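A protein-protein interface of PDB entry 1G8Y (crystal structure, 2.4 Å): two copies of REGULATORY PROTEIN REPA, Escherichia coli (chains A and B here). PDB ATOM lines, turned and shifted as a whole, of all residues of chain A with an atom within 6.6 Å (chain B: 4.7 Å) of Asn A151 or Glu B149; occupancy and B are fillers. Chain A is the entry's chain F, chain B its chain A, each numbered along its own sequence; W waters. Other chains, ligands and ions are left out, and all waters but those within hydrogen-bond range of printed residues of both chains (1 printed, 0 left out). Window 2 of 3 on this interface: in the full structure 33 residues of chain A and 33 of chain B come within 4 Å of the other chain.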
ATOM      1  N   GLU A 148     -18.360  -9.054  18.435  1.00  0.00           N
ATOM      2  CA  GLU A 148     -18.124  -7.739  17.852  1.00  0.00           C
ATOM      3  C   GLU A 148     -19.457  -7.028  17.502  1.00  0.00           C
ATOM      4  O   GLU A 148     -20.556  -7.628  17.508  1.00  0.00           O
ATOM      5  CB  GLU A 148     -17.279  -7.885  16.576  1.00  0.00           C
ATOM      6  CG  GLU A 148     -15.940  -8.635  16.729  1.00  0.00           C
ATOM      7  CD  GLU A 148     -15.129  -8.150  17.896  1.00  0.00           C
ATOM      8  OE1 GLU A 148     -15.194  -6.932  18.180  1.00  0.00           O
ATOM      9  OE2 GLU A 148     -14.429  -8.969  18.534  1.00  0.00           O
ATOM     10  N   GLU A 149     -19.337  -5.739  17.207  1.00  0.00           N
ATOM     11  CA  GLU A 149     -20.443  -4.878  16.788  1.00  0.00           C
ATOM     12  C   GLU A 149     -20.653  -5.274  15.316  1.00  0.00           C
ATOM     13  O   GLU A 149     -19.743  -5.099  14.508  1.00  0.00           O
ATOM     14  CB  GLU A 149     -19.958  -3.425  16.885  1.00  0.00           C
ATOM     15  CG  GLU A 149     -21.031  -2.377  16.901  1.00  0.00           C
ATOM     16  CD  GLU A 149     -21.968  -2.510  18.089  1.00  0.00           C
ATOM     17  OE1 GLU A 149     -21.483  -2.699  19.236  1.00  0.00           O
ATOM     18  OE2 GLU A 149     -23.193  -2.421  17.864  1.00  0.00           O
ATOM     19  N   GLU A 150     -21.810  -5.818  14.956  1.00  0.00           N
ATOM     20  CA  GLU A 150     -22.017  -6.242  13.570  1.00  0.00           C
ATOM     21  C   GLU A 150     -22.072  -5.089  12.580  1.00  0.00           C
ATOM     22  O   GLU A 150     -22.111  -5.305  11.366  1.00  0.00           O
ATOM     23  CB  GLU A 150     -23.266  -7.132  13.436  1.00  0.00           C
ATOM     24  CG  GLU A 150     -23.171  -8.435  14.247  1.00  0.00           C
ATOM     25  CD  GLU A 150     -23.942  -9.631  13.658  1.00  0.00           C
ATOM     26  OE1 GLU A 150     -25.106  -9.459  13.204  1.00  0.00           O
ATOM     27  OE2 GLU A 150     -23.378 -10.757  13.675  1.00  0.00           O
ATOM     28  N   ASN A 151     -22.043  -3.862  13.097  1.00  0.00           N
ATOM     29  CA  ASN A 151     -22.063  -2.675  12.246  1.00  0.00           C
ATOM     30  C   ASN A 151     -20.671  -2.093  12.027  1.00  0.00           C
ATOM     31  O   ASN A 151     -20.492  -1.162  11.242  1.00  0.00           O
ATOM     32  CB  ASN A 151     -22.957  -1.600  12.857  1.00  0.00           C
ATOM     33  CG  ASN A 151     -24.408  -1.974  12.808  1.00  0.00           C
ATOM     34  OD1 ASN A 151     -24.910  -2.414  11.766  1.00  0.00           O
ATOM     35  ND2 ASN A 151     -25.106  -1.805  13.930  1.00  0.00           N
ATOM     36  N   ALA A 152     -19.690  -2.627  12.742  1.00  0.00           N
ATOM     37  CA  ALA A 152     -18.325  -2.154  12.607  1.00  0.00           C
ATOM     38  C   ALA A 152     -17.587  -3.021  11.569  1.00  0.00           C
ATOM     39  O   ALA A 152     -17.288  -4.182  11.833  1.00  0.00           O
ATOM     40  CB  ALA A 152     -17.632  -2.211  13.952  1.00  0.00           C
ATOM     41  N   SER A 153     -17.312  -2.443  10.395  1.00  0.00           N
ATOM     42  CA  SER A 153     -16.630  -3.137   9.299  1.00  0.00           C
ATOM     43  C   SER A 153     -15.238  -3.683   9.640  1.00  0.00           C
ATOM     44  O   SER A 153     -14.862  -4.744   9.156  1.00  0.00           O
ATOM     45  CB  SER A 153     -16.530  -2.212   8.071  1.00  0.00           C
ATOM     46  OG  SER A 153     -15.784  -1.033   8.357  1.00  0.00           O
ATOM     47  N   GLY A 154     -14.472  -2.956  10.456  1.00  0.00           N
ATOM     48  CA  GLY A 154     -13.144  -3.430  10.831  1.00  0.00           C
ATOM     49  C   GLY A 154     -13.250  -4.754  11.605  1.00  0.00           C
ATOM     50  O   GLY A 154     -12.685  -5.785  11.206  1.00  0.00           O
ATOM     51  N   PRO A 155     -13.981  -4.764  12.729  1.00  0.00           N
ATOM     52  CA  PRO A 155     -14.086  -6.038  13.466  1.00  0.00           C
ATOM     53  C   PRO A 155     -14.726  -7.126  12.587  1.00  0.00           C
ATOM     54  O   PRO A 155     -14.269  -8.278  12.562  1.00  0.00           O
ATOM     55  CB  PRO A 155     -14.933  -5.671  14.694  1.00  0.00           C
ATOM     56  CG  PRO A 155     -14.609  -4.167  14.901  1.00  0.00           C
ATOM     57  CD  PRO A 155     -14.585  -3.638  13.472  1.00  0.00           C
ATOM     58  N   MET A 156     -15.764  -6.768  11.835  1.00  0.00           N
ATOM     59  CA  MET A 156     -16.393  -7.771  10.988  1.00  0.00           C
ATOM     60  C   MET A 156     -15.456  -8.265   9.888  1.00  0.00           C
ATOM     61  O   MET A 156     -15.575  -9.404   9.425  1.00  0.00           O
ATOM     62  CB  MET A 156     -17.709  -7.246  10.402  1.00  0.00           C
ATOM     63  CG  MET A 156     -18.793  -7.015  11.453  1.00  0.00           C
ATOM     64  SD  MET A 156     -18.958  -8.313  12.735  1.00  0.00           S
ATOM     65  CE  MET A 156     -19.476  -9.703  11.706  1.00  0.00           C
ATOM     66  N   VAL A 201     -21.923  -2.839   6.560  1.00  0.00           N
ATOM     67  CA  VAL A 201     -22.607  -4.060   6.145  1.00  0.00           C
ATOM     68  C   VAL A 201     -21.618  -5.172   5.811  1.00  0.00           C
ATOM     69  O   VAL A 201     -20.602  -4.941   5.157  1.00  0.00           O
ATOM     70  CB  VAL A 201     -23.506  -3.810   4.910  1.00  0.00           C
ATOM     71  CG1 VAL A 201     -24.566  -2.770   5.243  1.00  0.00           C
ATOM     72  CG2 VAL A 201     -22.663  -3.345   3.740  1.00  0.00           C
ATOM     73  N   ILE B 147      -7.679  -3.642   8.948  1.00  0.00           N
ATOM     74  CA  ILE B 147      -8.796  -3.961   9.842  1.00  0.00           C
ATOM     75  C   ILE B 147      -9.462  -2.708  10.441  1.00  0.00           C
ATOM     76  O   ILE B 147     -10.204  -2.805  11.414  1.00  0.00           O
ATOM     77  CB  ILE B 147      -8.325  -4.871  11.000  1.00  0.00           C
ATOM     78  CG1 ILE B 147      -7.283  -4.131  11.853  1.00  0.00           C
ATOM     79  CG2 ILE B 147      -7.721  -6.164  10.442  1.00  0.00           C
ATOM     80  CD1 ILE B 147      -6.800  -4.946  13.063  1.00  0.00           C
ATOM     81  N   GLU B 148      -9.204  -1.544   9.856  1.00  0.00           N
ATOM     82  CA  GLU B 148      -9.797  -0.312  10.360  1.00  0.00           C
ATOM     83  C   GLU B 148     -11.231  -0.084   9.841  1.00  0.00           C
ATOM     84  O   GLU B 148     -11.701  -0.744   8.914  1.00  0.00           O
ATOM     85  CB  GLU B 148      -8.935   0.903   9.970  1.00  0.00           C
ATOM     86  CG  GLU B 148      -7.445   0.756  10.227  1.00  0.00           C
ATOM     87  CD  GLU B 148      -7.153   0.393  11.663  1.00  0.00           C
ATOM     88  OE1 GLU B 148      -7.963   0.799  12.533  1.00  0.00           O
ATOM     89  OE2 GLU B 148      -6.116  -0.286  11.921  1.00  0.00           O
ATOM     90  N   GLU B 149     -11.912   0.863  10.468  1.00  0.00           N
ATOM     91  CA  GLU B 149     -13.276   1.242  10.102  1.00  0.00           C
ATOM     92  C   GLU B 149     -13.161   2.092   8.828  1.00  0.00           C
ATOM     93  O   GLU B 149     -12.588   3.183   8.867  1.00  0.00           O
ATOM     94  CB  GLU B 149     -13.864   2.090  11.241  1.00  0.00           C
ATOM     95  CG  GLU B 149     -15.363   2.038  11.407  1.00  0.00           C
ATOM     96  CD  GLU B 149     -15.870   0.618  11.571  1.00  0.00           C
ATOM     97  OE1 GLU B 149     -15.343  -0.135  12.434  1.00  0.00           O
ATOM     98  OE2 GLU B 149     -16.799   0.265  10.819  1.00  0.00           O
ATOM     99  N   GLU B 150     -13.681   1.601   7.701  1.00  0.00           N
ATOM    100  CA  GLU B 150     -13.605   2.354   6.447  1.00  0.00           C
ATOM    101  C   GLU B 150     -14.350   3.693   6.486  1.00  0.00           C
ATOM    102  O   GLU B 150     -14.245   4.489   5.557  1.00  0.00           O
ATOM    103  CB  GLU B 150     -14.053   1.489   5.242  1.00  0.00           C
ATOM    104  CG  GLU B 150     -13.033   0.356   4.959  1.00  0.00           C
ATOM    105  CD  GLU B 150     -13.130  -0.328   3.578  1.00  0.00           C
ATOM    106  OE1 GLU B 150     -14.247  -0.393   2.994  1.00  0.00           O
ATOM    107  OE2 GLU B 150     -12.064  -0.828   3.100  1.00  0.00           O
ATOM    108  N   ASN B 151     -15.061   3.955   7.580  1.00  0.00           N
ATOM    109  CA  ASN B 151     -15.774   5.221   7.753  1.00  0.00           C
ATOM    110  C   ASN B 151     -14.964   6.222   8.561  1.00  0.00           C
ATOM    111  O   ASN B 151     -15.256   7.418   8.525  1.00  0.00           O
ATOM    112  CB  ASN B 151     -17.106   5.020   8.481  1.00  0.00           C
ATOM    113  CG  ASN B 151     -18.102   4.264   7.649  1.00  0.00           C
ATOM    114  OD1 ASN B 151     -18.271   4.558   6.463  1.00  0.00           O
ATOM    115  ND2 ASN B 151     -18.779   3.287   8.258  1.00  0.00           N
ATOM    116  N   ALA B 152     -13.963   5.740   9.300  1.00  0.00           N
ATOM    117  CA  ALA B 152     -13.147   6.613  10.138  1.00  0.00           C
ATOM    118  C   ALA B 152     -11.966   7.216   9.372  1.00  0.00           C
ATOM    119  O   ALA B 152     -10.979   6.534   9.069  1.00  0.00           O
ATOM    120  CB  ALA B 152     -12.665   5.861  11.352  1.00  0.00           C
ATOM    121  N   MET B 156      -8.249   5.550   8.150  1.00  0.00           N
ATOM    122  CA  MET B 156      -8.109   5.415   6.712  1.00  0.00           C
ATOM    123  C   MET B 156      -6.994   6.301   6.202  1.00  0.00           C
ATOM    124  O   MET B 156      -6.323   5.960   5.228  1.00  0.00           O
ATOM    125  CB  MET B 156      -9.410   5.742   6.003  1.00  0.00           C
ATOM    126  CG  MET B 156     -10.489   4.692   6.211  1.00  0.00           C
ATOM    127  SD  MET B 156      -9.847   2.996   6.249  1.00  0.00           S
ATOM    128  CE  MET B 156      -9.345   2.809   4.598  1.00  0.00           C
HETATM  129  O   HOH W   1     -15.690  -1.137   4.895  1.00  0.00           O
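The side-chain carboxylate of Glu B149 lies within hydrogen-bond range of the backbone NH of Ser A153.
N of Glu B150 is in hydrogen-bond range of OG of Ser A153 (3.4 Å).
Water W1 lies within hydrogen-bond range of the side-chain carboxylate of Glu B150 (2.5 Å) and the side-chain hydroxyl of Ser A153 (3.5 Å).
Asn A151 touches Glu B149, but with the chains exchanged Glu A149 does not touch Asn B151 (10.5 Å).
Ala A152 touches Glu B149, but with the chains exchanged Glu A149 does not touch Ala B152 (13.0 Å).
Of the 8 pairs that touch across the chains among the printed residues, none has its exchanged pair printed and touching as well.
Among the printed residues, merely in contact across the chains: Asn A151 with Glu B149 (3.98 Å), Ala A152 with Glu B149 (3.4 Å), Gly A154 with Ile B147 (3.1 Å), Gly A154 with Glu B148 (3.6 Å), Gly A154 with Glu B149 (3.6 Å) and Pro A155 with Glu B149 (3.7 Å).
Along chain A the printed residues that touch a printed residue of chain B span positions 151 to 155.
Of the 7 printed residues of chain B, 4 touch a printed residue of chain A.
Among the printed residues, 8 pairs touch across the chains.
Of the printed residues of chain B, Asn A151 touches Glu B149 (3.98 Å).
Printed residues of chain B within 4 Å of Ser A153: Glu B149 and Glu B150.
Printed residues of chain B within 4 Å of Gly A154: Ile B147 (3.1 Å), Glu B148 (3.6 Å) and Glu B149 (3.6 Å).
Printed residues of chain A within 4 Å of Ile B147: Gly A154 (3.1 Å).
Printed residues of chain A within 4 Å of Glu B148: Gly A154 (3.6 Å).
The nearest printed residue of chain A that does not touch Glu B149 is Met A156 (6.7 Å).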
